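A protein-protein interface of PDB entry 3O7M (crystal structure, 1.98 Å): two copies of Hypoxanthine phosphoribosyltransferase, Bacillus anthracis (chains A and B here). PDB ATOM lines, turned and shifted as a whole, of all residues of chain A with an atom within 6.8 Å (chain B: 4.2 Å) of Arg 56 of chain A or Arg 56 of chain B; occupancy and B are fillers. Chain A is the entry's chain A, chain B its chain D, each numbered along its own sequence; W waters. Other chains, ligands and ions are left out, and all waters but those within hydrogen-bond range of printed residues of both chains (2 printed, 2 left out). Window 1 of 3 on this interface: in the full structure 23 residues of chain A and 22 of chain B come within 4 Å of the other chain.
The backbone carbonyl oxygen (O) of Ile 58 of chain B sits at hydrogen-bond distance from the side-chain amide nitrogen (ND2) of Asn 168 of chain A. The side-chain carboxylate (OD2) of Asp 53 of chain B is in salt-bridge range of the guanidinium group (NH1) of Arg 56 of chain A. O of Ile 55 of chain A lies close to O of Asn 168 of chain B, 3.5 Å away. The guanidinium group of Arg 56 of chain B lies within salt-bridge range of the side-chain carboxylate of Asp 53 of chain A. ND2 of Asn 168 of chain B sits at hydrogen-bond distance from O of Ile 58 of chain A, 3.0 Å away.
NZ of Lys 59 of chain A sits at hydrogen-bond distance from O of Arg 56 of chain A, at 2.8 Å. O of Arg 56 of chain B is in hydrogen-bond range of NZ of Lys 59 of chain B (2.8 Å). O of Leu 169 of chain A is in hydrogen-bond range of N of Tyr 158 of chain A (2.9 Å). The side-chain hydroxyl of Tyr 158 of chain B is in hydrogen-bond range of the side-chain carboxylate of Asp 53 of chain B. OH of Tyr 158 of chain A lies within hydrogen-bond range of OD2 of Asp 53 of chain A (2.8 Å). OD1 of Asp 53 of chain B is in salt-bridge range of NH2 of Arg 56 of chain B, 2.8 Å away.
NH1 of Arg 56 of chain B touches NE2 of Gln 19 of chain A (3.8 Å). Arg 56 of chain B touches Val 49 of chain A. Ala 52 of chain B touches Ala 52 of chain A. CG1 of Val 49 of chain B touches CZ of Arg 56 of chain A, at 3.5 Å. NH2 of Arg 56 of chain A touches NH2 of Arg 56 of chain B, at 3.9 Å. Arg 56 of chain A touches Tyr 158 of chain B (NH1 to CE1, 3.4 Å). Asn 168 of chain B touches Arg 56 of chain A (O to CA, 3.5 Å). Tyr 158 of chain A touches Arg 56 of chain B (CE1 to NH1, 3.4 Å). Asn 168 of chain A touches Ile 55 of chain B (CB to O, 3.3 Å). Lys 59 of chain B touches Pro 170 of chain A (NZ to CG, 3.9 Å).
Leu 18 of chain A touches none of the printed residues of chain B. Arg 56 of chain A touches just these residues of chain B: Val 49, Asp 53, Arg 56, Tyr 158 and Asn 168. Of the printed residues of chain B, Tyr 158 of chain A touches Arg 56 (3.4 Å). Of the printed residues of chain A, Val 49 of chain B touches Arg 56. Printed residues of chain A within 4 Å of Ile 55 of chain B: Asn 168. Of the printed residues of chain A, Arg 56 of chain B touches Gln 19 (3.8 Å), Val 49 (3.5 Å), Asp 53 (2.7 Å), Arg 56 (3.9 Å), Tyr 158 (3.4 Å) and Asn 168 (3.5 Å). Printed residues of chain A within 4 Å of Ile 58 of chain B: Asn 168 (2.9 Å). The nearest residue of chain B that does not touch Arg 56 of chain A is Pro 170 of chain B (4.1 Å). The nearest printed residue of chain A that does not touch Arg 56 of chain B is Pro 170 of chain A (4.2 Å). The nearest printed residue of chain B that does not touch Tyr 158 of chain A is Ile 55 of chain B (6.9 Å).
Of the 12 printed residues of chain B, 9 touch a printed residue of chain A. Hydrophobic or aromatic side chains of chain B that line the printed part of chain A: Val 49, Ala 52, Ile 55 and Tyr 158. Printed residues of chain A that touch a printed residue of chain B: Gln 19, Val 49, Ala 52, Asp 53, Ile 55, Arg 56, Ile 58, Tyr 158, Asn 168 and Pro 170. Hydrophobic or aromatic side chains of chain A within 4 Å of the printed part of chain B: Val 49, Ala 52, Tyr 158 and Pro 170.
Asp 53 of chain A touches Arg 56 of chain B, and with the chains exchanged Arg 56 of chain A touches Asp 53 of chain B. Arg 56 of chain A touches Asn 168 of chain B, and with the chains exchanged Asn 168 of chain A touches Arg 56 of chain B. Ile 58 of chain A touches Asn 168 of chain B, and with the chains exchanged Asn 168 of chain A touches Ile 58 of chain B. Pro 170 of chain A touches Lys 59 of chain B, but with the chains exchanged Lys 59 of chain A does not touch Pro 170 of chain B (4.1 Å). Positions printed for both chains: 49, 52, 53, 54, 55, 56, 57, 58, 59, 158, 168 and 170. Of the 16 pairs that touch across the chains among the printed residues, 14 have their exchanged pair printed and touching as well.
Water W2 lies within hydrogen-bond range of O of Pro 170 of chain B and NH1 of Arg 56 of chain A. Water W1 lies within hydrogen-bond range of the backbone carbonyl oxygen (O) of Pro 170 of chain A, the side-chain amide nitrogen (NE2) of Gln 19 of chain A and the guanidinium group (NH1) of Arg 56 of chain B.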
ATOM      1  N   GLU A  15      28.185 -30.972  18.691  1.00  0.00           N
ATOM      2  CA  GLU A  15      27.319 -29.855  18.294  1.00  0.00           C
ATOM      3  C   GLU A  15      25.853 -30.132  18.685  1.00  0.00           C
ATOM      4  O   GLU A  15      25.135 -29.276  19.226  1.00  0.00           O
ATOM      5  CB  GLU A  15      27.441 -29.661  16.767  1.00  0.00           C
ATOM      6  CG  GLU A  15      26.689 -28.477  16.226  1.00  0.00           C
ATOM      7  CD  GLU A  15      26.872 -28.304  14.717  1.00  0.00           C
ATOM      8  OE1 GLU A  15      27.602 -29.092  14.113  1.00  0.00           O
ATOM      9  OE2 GLU A  15      26.281 -27.382  14.141  1.00  0.00           O
ATOM     10  N   LEU A  18      25.374 -29.992  22.500  1.00  0.00           N
ATOM     11  CA  LEU A  18      25.334 -28.602  22.892  1.00  0.00           C
ATOM     12  C   LEU A  18      23.974 -27.975  22.609  1.00  0.00           C
ATOM     13  O   LEU A  18      23.417 -27.279  23.467  1.00  0.00           O
ATOM     14  CB  LEU A  18      26.420 -27.771  22.195  1.00  0.00           C
ATOM     15  CG  LEU A  18      27.827 -28.008  22.691  1.00  0.00           C
ATOM     16  CD1 LEU A  18      28.882 -27.446  21.672  1.00  0.00           C
ATOM     17  CD2 LEU A  18      28.043 -27.435  24.095  1.00  0.00           C
ATOM     18  N   GLN A  19      23.422 -28.197  21.430  1.00  0.00           N
ATOM     19  CA  GLN A  19      22.147 -27.571  21.126  1.00  0.00           C
ATOM     20  C   GLN A  19      21.021 -28.159  22.011  1.00  0.00           C
ATOM     21  O   GLN A  19      20.135 -27.421  22.440  1.00  0.00           O
ATOM     22  CB  GLN A  19      21.815 -27.625  19.639  1.00  0.00           C
ATOM     23  CG  GLN A  19      22.920 -27.154  18.673  1.00  0.00           C
ATOM     24  CD  GLN A  19      23.720 -25.878  19.079  1.00  0.00           C
ATOM     25  OE1 GLN A  19      23.359 -25.137  19.997  1.00  0.00           O
ATOM     26  NE2 GLN A  19      24.798 -25.614  18.334  1.00  0.00           N
ATOM     27  N   VAL A  22      21.490 -26.382  25.419  1.00  0.00           N
ATOM     28  CA  VAL A  22      21.074 -25.007  25.345  1.00  0.00           C
ATOM     29  C   VAL A  22      19.562 -24.871  25.407  1.00  0.00           C
ATOM     30  O   VAL A  22      19.037 -23.980  26.082  1.00  0.00           O
ATOM     31  CB  VAL A  22      21.609 -24.360  24.056  1.00  0.00           C
ATOM     32  CG1 VAL A  22      20.900 -23.051  23.798  1.00  0.00           C
ATOM     33  CG2 VAL A  22      23.138 -24.157  24.152  1.00  0.00           C
ATOM     34  N   ALA A  26      17.483 -22.920  28.333  1.00  0.00           N
ATOM     35  CA  ALA A  26      16.525 -21.869  27.935  1.00  0.00           C
ATOM     36  C   ALA A  26      15.127 -22.161  28.476  1.00  0.00           C
ATOM     37  O   ALA A  26      14.439 -21.251  28.981  1.00  0.00           O
ATOM     38  CB  ALA A  26      16.482 -21.701  26.404  1.00  0.00           C
ATOM     39  N   VAL A  49      29.162 -17.125  21.925  1.00  0.00           N
ATOM     40  CA  VAL A  49      28.505 -18.143  21.072  1.00  0.00           C
ATOM     41  C   VAL A  49      27.347 -18.791  21.831  1.00  0.00           C
ATOM     42  O   VAL A  49      26.215 -18.872  21.345  1.00  0.00           O
ATOM     43  CB  VAL A  49      29.519 -19.157  20.579  1.00  0.00           C
ATOM     44  CG1 VAL A  49      28.842 -20.283  19.799  1.00  0.00           C
ATOM     45  CG2 VAL A  49      30.589 -18.455  19.684  1.00  0.00           C
ATOM     46  N   PHE A  50      27.637 -19.211  23.064  1.00  0.00           N
ATOM     47  CA  PHE A  50      26.649 -19.778  23.955  1.00  0.00           C
ATOM     48  C   PHE A  50      25.492 -18.790  24.119  1.00  0.00           C
ATOM     49  O   PHE A  50      24.333 -19.170  24.069  1.00  0.00           O
ATOM     50  CB  PHE A  50      27.323 -20.097  25.299  1.00  0.00           C
ATOM     51  CG  PHE A  50      26.404 -20.600  26.401  1.00  0.00           C
ATOM     52  CD1 PHE A  50      25.403 -21.526  26.150  1.00  0.00           C
ATOM     53  CD2 PHE A  50      26.602 -20.177  27.717  1.00  0.00           C
ATOM     54  CE1 PHE A  50      24.590 -21.974  27.176  1.00  0.00           C
ATOM     55  CE2 PHE A  50      25.847 -20.686  28.768  1.00  0.00           C
ATOM     56  CZ  PHE A  50      24.825 -21.599  28.494  1.00  0.00           C
ATOM     57  N   ALA A  51      25.814 -17.530  24.364  1.00  0.00           N
ATOM     58  CA  ALA A  51      24.788 -16.502  24.549  1.00  0.00           C
ATOM     59  C   ALA A  51      23.896 -16.337  23.332  1.00  0.00           C
ATOM     60  O   ALA A  51      22.687 -16.255  23.458  1.00  0.00           O
ATOM     61  CB  ALA A  51      25.419 -15.149  24.967  1.00  0.00           C
ATOM     62  N   ALA A  52      24.513 -16.302  22.170  1.00  0.00           N
ATOM     63  CA  ALA A  52      23.814 -16.153  20.890  1.00  0.00           C
ATOM     64  C   ALA A  52      22.796 -17.288  20.721  1.00  0.00           C
ATOM     65  O   ALA A  52      21.658 -17.049  20.319  1.00  0.00           O
ATOM     66  CB  ALA A  52      24.809 -16.150  19.757  1.00  0.00           C
ATOM     67  N   ASP A  53      23.221 -18.501  21.032  1.00  0.00           N
ATOM     68  CA  ASP A  53      22.372 -19.685  20.907  1.00  0.00           C
ATOM     69  C   ASP A  53      21.319 -19.722  21.984  1.00  0.00           C
ATOM     70  O   ASP A  53      20.154 -20.024  21.723  1.00  0.00           O
ATOM     71  CB  ASP A  53      23.214 -20.948  20.953  1.00  0.00           C
ATOM     72  CG  ASP A  53      23.985 -21.196  19.644  1.00  0.00           C
ATOM     73  OD1 ASP A  53      23.842 -20.416  18.674  1.00  0.00           O
ATOM     74  OD2 ASP A  53      24.763 -22.161  19.625  1.00  0.00           O
ATOM     75  N   LEU A  54      21.716 -19.400  23.200  1.00  0.00           N
ATOM     76  CA  LEU A  54      20.789 -19.450  24.311  1.00  0.00           C
ATOM     77  C   LEU A  54      19.612 -18.479  24.144  1.00  0.00           C
ATOM     78  O   LEU A  54      18.445 -18.868  24.296  1.00  0.00           O
ATOM     79  CB  LEU A  54      21.515 -19.134  25.605  1.00  0.00           C
ATOM     80  CG  LEU A  54      20.713 -19.228  26.900  1.00  0.00           C
ATOM     81  CD1 LEU A  54      20.341 -20.692  27.201  1.00  0.00           C
ATOM     82  CD2 LEU A  54      21.527 -18.584  28.046  1.00  0.00           C
ATOM     83  N   ILE A  55      19.913 -17.229  23.824  1.00  0.00           N
ATOM     84  CA  ILE A  55      18.838 -16.249  23.715  1.00  0.00           C
ATOM     85  C   ILE A  55      17.832 -16.533  22.603  1.00  0.00           C
ATOM     86  O   ILE A  55      16.655 -16.130  22.691  1.00  0.00           O
ATOM     87  CB  ILE A  55      19.327 -14.787  23.620  1.00  0.00           C
ATOM     88  CG1 ILE A  55      20.056 -14.535  22.311  1.00  0.00           C
ATOM     89  CG2 ILE A  55      20.166 -14.446  24.849  1.00  0.00           C
ATOM     90  CD1 ILE A  55      20.432 -13.036  22.124  1.00  0.00           C
ATOM     91  N   ARG A  56      18.261 -17.240  21.585  1.00  0.00           N
ATOM     92  CA  ARG A  56      17.384 -17.597  20.501  1.00  0.00           C
ATOM     93  C   ARG A  56      16.404 -18.708  20.895  1.00  0.00           C
ATOM     94  O   ARG A  56      15.517 -19.063  20.097  1.00  0.00           O
ATOM     95  CB  ARG A  56      18.202 -17.938  19.257  1.00  0.00           C
ATOM     96  CG  ARG A  56      18.744 -16.667  18.599  1.00  0.00           C
ATOM     97  CD  ARG A  56      19.452 -17.010  17.306  1.00  0.00           C
ATOM     98  NE  ARG A  56      20.769 -17.562  17.598  1.00  0.00           N
ATOM     99  CZ  ARG A  56      21.644 -17.907  16.673  1.00  0.00           C
ATOM    100  NH1 ARG A  56      21.339 -17.783  15.381  1.00  0.00           N
ATOM    101  NH2 ARG A  56      22.840 -18.333  17.037  1.00  0.00           N
ATOM    102  N   HIS A  57      16.534 -19.261  22.099  1.00  0.00           N
ATOM    103  CA  HIS A  57      15.513 -20.228  22.584  1.00  0.00           C
ATOM    104  C   HIS A  57      14.735 -19.672  23.748  1.00  0.00           C
ATOM    105  O   HIS A  57      13.895 -20.340  24.308  1.00  0.00           O
ATOM    106  CB  HIS A  57      16.127 -21.551  22.979  1.00  0.00           C
ATOM    107  CG  HIS A  57      16.679 -22.283  21.812  1.00  0.00           C
ATOM    108  ND1 HIS A  57      15.873 -22.948  20.919  1.00  0.00           N
ATOM    109  CD2 HIS A  57      17.936 -22.362  21.325  1.00  0.00           C
ATOM    110  CE1 HIS A  57      16.625 -23.477  19.966  1.00  0.00           C
ATOM    111  NE2 HIS A  57      17.879 -23.128  20.184  1.00  0.00           N
ATOM    112  N   ILE A  58      15.046 -18.445  24.138  1.00  0.00           N
ATOM    113  CA  ILE A  58      14.321 -17.806  25.223  1.00  0.00           C
ATOM    114  C   ILE A  58      13.321 -16.850  24.574  1.00  0.00           C
ATOM    115  O   ILE A  58      13.724 -15.899  23.878  1.00  0.00           O
ATOM    116  CB  ILE A  58      15.270 -17.020  26.122  1.00  0.00           C
ATOM    117  CG1 ILE A  58      16.194 -17.981  26.865  1.00  0.00           C
ATOM    118  CG2 ILE A  58      14.435 -16.177  27.150  1.00  0.00           C
ATOM    119  CD1 ILE A  58      17.345 -17.207  27.639  1.00  0.00           C
ATOM    120  N   LYS A  59      12.043 -17.099  24.780  1.00  0.00           N
ATOM    121  CA  LYS A  59      11.010 -16.278  24.171  1.00  0.00           C
ATOM    122  C   LYS A  59      10.546 -15.093  24.974  1.00  0.00           C
ATOM    123  O   LYS A  59       9.815 -14.247  24.439  1.00  0.00           O
ATOM    124  CB  LYS A  59       9.826 -17.132  23.751  1.00  0.00           C
ATOM    125  CG  LYS A  59      10.256 -18.317  22.855  1.00  0.00           C
ATOM    126  CD  LYS A  59      11.185 -17.945  21.714  1.00  0.00           C
ATOM    127  CE  LYS A  59      11.810 -19.194  20.977  1.00  0.00           C
ATOM    128  NZ  LYS A  59      12.737 -18.839  19.827  1.00  0.00           N
ATOM    129  N   TYR A 158      33.356 -23.723  20.586  1.00  0.00           N
ATOM    130  CA  TYR A 158      32.052 -23.073  20.846  1.00  0.00           C
ATOM    131  C   TYR A 158      32.263 -21.774  21.651  1.00  0.00           C
ATOM    132  O   TYR A 158      31.621 -21.567  22.665  1.00  0.00           O
ATOM    133  CB  TYR A 158      31.211 -24.050  21.652  1.00  0.00           C
ATOM    134  CG  TYR A 158      29.724 -23.744  21.779  1.00  0.00           C
ATOM    135  CD1 TYR A 158      28.865 -23.974  20.729  1.00  0.00           C
ATOM    136  CD2 TYR A 158      29.173 -23.312  22.985  1.00  0.00           C
ATOM    137  CE1 TYR A 158      27.489 -23.732  20.851  1.00  0.00           C
ATOM    138  CE2 TYR A 158      27.807 -23.085  23.115  1.00  0.00           C
ATOM    139  CZ  TYR A 158      26.974 -23.280  22.039  1.00  0.00           C
ATOM    140  OH  TYR A 158      25.620 -23.024  22.141  1.00  0.00           O
ATOM    141  N   GLY A 159      33.165 -20.942  21.162  1.00  0.00           N
ATOM    142  CA  GLY A 159      33.516 -19.646  21.784  1.00  0.00           C
ATOM    143  C   GLY A 159      34.761 -19.642  22.651  1.00  0.00           C
ATOM    144  O   GLY A 159      35.376 -18.582  22.837  1.00  0.00           O
ATOM    145  N   ARG A 167      38.060 -21.038  18.879  1.00  0.00           N
ATOM    146  CA  ARG A 167      36.727 -20.540  19.253  1.00  0.00           C
ATOM    147  C   ARG A 167      35.685 -20.867  18.191  1.00  0.00           C
ATOM    148  O   ARG A 167      34.504 -20.939  18.496  1.00  0.00           O
ATOM    149  CB  ARG A 167      36.695 -19.040  19.445  1.00  0.00           C
ATOM    150  CG  ARG A 167      37.632 -18.487  20.488  1.00  0.00           C
ATOM    151  CD  ARG A 167      37.283 -17.043  20.727  1.00  0.00           C
ATOM    152  NE  ARG A 167      38.243 -16.305  21.542  1.00  0.00           N
ATOM    153  CZ  ARG A 167      38.201 -16.136  22.855  1.00  0.00           C
ATOM    154  NH1 ARG A 167      37.311 -16.754  23.604  1.00  0.00           N
ATOM    155  NH2 ARG A 167      39.137 -15.392  23.427  1.00  0.00           N
ATOM    156  N   ASN A 168      36.132 -21.043  16.951  1.00  0.00           N
ATOM    157  CA  ASN A 168      35.257 -21.363  15.836  1.00  0.00           C
ATOM    158  C   ASN A 168      34.745 -22.835  15.739  1.00  0.00           C
ATOM    159  O   ASN A 168      33.871 -23.164  14.903  1.00  0.00           O
ATOM    160  CB  ASN A 168      35.880 -20.948  14.521  1.00  0.00           C
ATOM    161  CG  ASN A 168      37.200 -21.617  14.236  1.00  0.00           C
ATOM    162  OD1 ASN A 168      38.009 -21.793  15.131  1.00  0.00           O
ATOM    163  ND2 ASN A 168      37.436 -21.985  12.960  1.00  0.00           N
ATOM    164  N   LEU A 169      35.268 -23.734  16.556  1.00  0.00           N
ATOM    165  CA  LEU A 169      34.778 -25.110  16.491  1.00  0.00           C
ATOM    166  C   LEU A 169      33.341 -25.155  16.886  1.00  0.00           C
ATOM    167  O   LEU A 169      32.950 -24.495  17.843  1.00  0.00           O
ATOM    168  CB  LEU A 169      35.554 -26.029  17.428  1.00  0.00           C
ATOM    169  CG  LEU A 169      37.034 -26.193  17.215  1.00  0.00           C
ATOM    170  CD1 LEU A 169      37.581 -27.109  18.348  1.00  0.00           C
ATOM    171  CD2 LEU A 169      37.388 -26.780  15.795  1.00  0.00           C
ATOM    172  N   PRO A 170      32.524 -25.950  16.177  1.00  0.00           N
ATOM    173  CA  PRO A 170      31.145 -25.994  16.601  1.00  0.00           C
ATOM    174  C   PRO A 170      30.861 -26.983  17.714  1.00  0.00           C
ATOM    175  O   PRO A 170      29.714 -27.146  18.100  1.00  0.00           O
ATOM    176  CB  PRO A 170      30.382 -26.409  15.338  1.00  0.00           C
ATOM    177  CG  PRO A 170      31.376 -26.981  14.448  1.00  0.00           C
ATOM    178  CD  PRO A 170      32.716 -26.491  14.821  1.00  0.00           C
ATOM    179  N   PHE A 171      31.893 -27.615  18.241  1.00  0.00           N
ATOM    180  CA  PHE A 171      31.731 -28.581  19.311  1.00  0.00           C
ATOM    181  C   PHE A 171      32.798 -28.213  20.320  1.00  0.00           C
ATOM    182  O   PHE A 171      33.653 -27.360  20.056  1.00  0.00           O
ATOM    183  CB  PHE A 171      31.929 -30.021  18.792  1.00  0.00           C
ATOM    184  CG  PHE A 171      33.212 -30.215  18.018  1.00  0.00           C
ATOM    185  CD1 PHE A 171      34.388 -30.588  18.652  1.00  0.00           C
ATOM    186  CD2 PHE A 171      33.241 -30.002  16.637  1.00  0.00           C
ATOM    187  CE1 PHE A 171      35.579 -30.705  17.927  1.00  0.00           C
ATOM    188  CE2 PHE A 171      34.428 -30.121  15.922  1.00  0.00           C
ATOM    189  CZ  PHE A 171      35.593 -30.484  16.581  1.00  0.00           C
ATOM    190  N   VAL B  49      25.525 -12.289  17.087  1.00  0.00           N
ATOM    191  CA  VAL B  49      24.798 -13.509  16.681  1.00  0.00           C
ATOM    192  C   VAL B  49      25.284 -13.992  15.300  1.00  0.00           C
ATOM    193  O   VAL B  49      25.640 -15.145  15.100  1.00  0.00           O
ATOM    194  CB  VAL B  49      23.278 -13.281  16.719  1.00  0.00           C
ATOM    195  CG1 VAL B  49      22.559 -14.518  16.216  1.00  0.00           C
ATOM    196  CG2 VAL B  49      22.800 -12.931  18.163  1.00  0.00           C
ATOM    197  N   ALA B  52      28.733 -15.352  15.611  1.00  0.00           N
ATOM    198  CA  ALA B  52      28.749 -16.674  16.227  1.00  0.00           C
ATOM    199  C   ALA B  52      28.400 -17.756  15.207  1.00  0.00           C
ATOM    200  O   ALA B  52      29.050 -18.824  15.141  1.00  0.00           O
ATOM    201  CB  ALA B  52      27.763 -16.725  17.402  1.00  0.00           C
ATOM    202  N   ASP B  53      27.419 -17.475  14.376  1.00  0.00           N
ATOM    203  CA  ASP B  53      27.009 -18.450  13.361  1.00  0.00           C
ATOM    204  C   ASP B  53      28.002 -18.529  12.222  1.00  0.00           C
ATOM    205  O   ASP B  53      28.316 -19.617  11.765  1.00  0.00           O
ATOM    206  CB  ASP B  53      25.644 -18.106  12.807  1.00  0.00           C
ATOM    207  CG  ASP B  53      24.533 -18.339  13.794  1.00  0.00           C
ATOM    208  OD1 ASP B  53      24.779 -18.867  14.911  1.00  0.00           O
ATOM    209  OD2 ASP B  53      23.401 -17.936  13.452  1.00  0.00           O
ATOM    210  N   LEU B  54      28.492 -17.376  11.769  1.00  0.00           N
ATOM    211  CA  LEU B  54      29.446 -17.319  10.672  1.00  0.00           C
ATOM    212  C   LEU B  54      30.742 -18.100  10.965  1.00  0.00           C
ATOM    213  O   LEU B  54      31.174 -18.936  10.164  1.00  0.00           O
ATOM    214  CB  LEU B  54      29.795 -15.870  10.350  1.00  0.00           C
ATOM    215  CG  LEU B  54      30.711 -15.622   9.142  1.00  0.00           C
ATOM    216  CD1 LEU B  54      29.963 -15.984   7.828  1.00  0.00           C
ATOM    217  CD2 LEU B  54      31.193 -14.176   9.114  1.00  0.00           C
ATOM    218  N   ILE B  55      31.338 -17.869  12.128  1.00  0.00           N
ATOM    219  CA  ILE B  55      32.633 -18.463  12.397  1.00  0.00           C
ATOM    220  C   ILE B  55      32.551 -19.984  12.539  1.00  0.00           C
ATOM    221  O   ILE B  55      33.530 -20.678  12.269  1.00  0.00           O
ATOM    222  CB  ILE B  55      33.380 -17.849  13.606  1.00  0.00           C
ATOM    223  CG1 ILE B  55      32.698 -18.184  14.934  1.00  0.00           C
ATOM    224  CG2 ILE B  55      33.615 -16.346  13.420  1.00  0.00           C
ATOM    225  CD1 ILE B  55      33.545 -17.835  16.131  1.00  0.00           C
ATOM    226  N   ARG B  56      31.388 -20.485  12.922  1.00  0.00           N
ATOM    227  CA  ARG B  56      31.162 -21.920  13.042  1.00  0.00           C
ATOM    228  C   ARG B  56      31.060 -22.617  11.698  1.00  0.00           C
ATOM    229  O   ARG B  56      30.982 -23.839  11.646  1.00  0.00           O
ATOM    230  CB  ARG B  56      29.965 -22.216  13.938  1.00  0.00           C
ATOM    231  CG  ARG B  56      30.332 -21.956  15.427  1.00  0.00           C
ATOM    232  CD  ARG B  56      29.168 -22.330  16.324  1.00  0.00           C
ATOM    233  NE  ARG B  56      28.144 -21.296  16.300  1.00  0.00           N
ATOM    234  CZ  ARG B  56      27.020 -21.334  17.000  1.00  0.00           C
ATOM    235  NH1 ARG B  56      26.740 -22.354  17.806  1.00  0.00           N
ATOM    236  NH2 ARG B  56      26.180 -20.329  16.916  1.00  0.00           N
ATOM    237  N   HIS B  57      31.069 -21.846  10.629  1.00  0.00           N
ATOM    238  CA  HIS B  57      31.106 -22.413   9.288  1.00  0.00           C
ATOM    239  C   HIS B  57      32.408 -22.142   8.592  1.00  0.00           C
ATOM    240  O   HIS B  57      32.563 -22.475   7.433  1.00  0.00           O
ATOM    241  CB  HIS B  57      29.939 -21.963   8.423  1.00  0.00           C
ATOM    242  CG  HIS B  57      28.643 -22.576   8.841  1.00  0.00           C
ATOM    243  ND1 HIS B  57      28.361 -23.905   8.623  1.00  0.00           N
ATOM    244  CD2 HIS B  57      27.587 -22.071   9.515  1.00  0.00           C
ATOM    245  CE1 HIS B  57      27.178 -24.193   9.140  1.00  0.00           C
ATOM    246  NE2 HIS B  57      26.692 -23.099   9.700  1.00  0.00           N
ATOM    247  N   ILE B  58      33.330 -21.504   9.279  1.00  0.00           N
ATOM    248  CA  ILE B  58      34.639 -21.203   8.692  1.00  0.00           C
ATOM    249  C   ILE B  58      35.635 -22.156   9.349  1.00  0.00           C
ATOM    250  O   ILE B  58      35.833 -22.112  10.582  1.00  0.00           O
ATOM    251  CB  ILE B  58      35.053 -19.770   8.985  1.00  0.00           C
ATOM    252  CG1 ILE B  58      34.140 -18.771   8.276  1.00  0.00           C
ATOM    253  CG2 ILE B  58      36.516 -19.540   8.545  1.00  0.00           C
ATOM    254  CD1 ILE B  58      34.370 -17.335   8.676  1.00  0.00           C
ATOM    255  N   LYS B  59      36.248 -23.025   8.563  1.00  0.00           N
ATOM    256  CA  LYS B  59      37.156 -24.016   9.123  1.00  0.00           C
ATOM    257  C   LYS B  59      38.614 -23.560   9.172  1.00  0.00           C
ATOM    258  O   LYS B  59      39.447 -24.246   9.773  1.00  0.00           O
ATOM    259  CB  LYS B  59      37.044 -25.383   8.420  1.00  0.00           C
ATOM    260  CG  LYS B  59      35.606 -25.985   8.415  1.00  0.00           C
ATOM    261  CD  LYS B  59      34.819 -25.656   9.678  1.00  0.00           C
ATOM    262  CE  LYS B  59      33.299 -25.969   9.584  1.00  0.00           C
ATOM    263  NZ  LYS B  59      32.593 -25.957  10.921  1.00  0.00           N
ATOM    264  N   TYR B 158      17.823 -11.431  15.368  1.00  0.00           N
ATOM    265  CA  TYR B 158      19.111 -12.021  15.026  1.00  0.00           C
ATOM    266  C   TYR B 158      20.247 -11.108  15.450  1.00  0.00           C
ATOM    267  O   TYR B 158      21.189 -10.872  14.686  1.00  0.00           O
ATOM    268  CB  TYR B 158      19.178 -12.292  13.512  1.00  0.00           C
ATOM    269  CG  TYR B 158      20.275 -13.257  13.073  1.00  0.00           C
ATOM    270  CD1 TYR B 158      20.191 -14.611  13.343  1.00  0.00           C
ATOM    271  CD2 TYR B 158      21.365 -12.821  12.334  1.00  0.00           C
ATOM    272  CE1 TYR B 158      21.163 -15.524  12.862  1.00  0.00           C
ATOM    273  CE2 TYR B 158      22.338 -13.710  11.891  1.00  0.00           C
ATOM    274  CZ  TYR B 158      22.243 -15.047  12.164  1.00  0.00           C
ATOM    275  OH  TYR B 158      23.253 -15.905  11.737  1.00  0.00           O
ATOM    276  N   ASN B 168      16.769 -11.246  20.493  1.00  0.00           N
ATOM    277  CA  ASN B 168      16.623 -12.684  20.661  1.00  0.00           C
ATOM    278  C   ASN B 168      15.774 -13.429  19.616  1.00  0.00           C
ATOM    279  O   ASN B 168      15.715 -14.672  19.654  1.00  0.00           O
ATOM    280  CB  ASN B 168      16.087 -13.017  22.069  1.00  0.00           C
ATOM    281  CG  ASN B 168      14.762 -12.357  22.351  1.00  0.00           C
ATOM    282  OD1 ASN B 168      14.568 -11.215  21.957  1.00  0.00           O
ATOM    283  ND2 ASN B 168      13.833 -13.066  22.995  1.00  0.00           N
ATOM    284  N   PRO B 170      14.976 -15.360  16.406  1.00  0.00           N
ATOM    285  CA  PRO B 170      15.897 -16.095  15.544  1.00  0.00           C
ATOM    286  C   PRO B 170      15.773 -15.768  14.056  1.00  0.00           C
ATOM    287  O   PRO B 170      16.430 -16.406  13.226  1.00  0.00           O
ATOM    288  CB  PRO B 170      15.519 -17.547  15.793  1.00  0.00           C
ATOM    289  CG  PRO B 170      14.128 -17.517  16.257  1.00  0.00           C
ATOM    290  CD  PRO B 170      13.859 -16.193  16.875  1.00  0.00           C
HETATM  291  O   HOH W   1      27.683 -25.279  17.635  1.00  0.00           O
HETATM  292  O   HOH W   2      18.705 -17.748  13.934  1.00  0.00           O
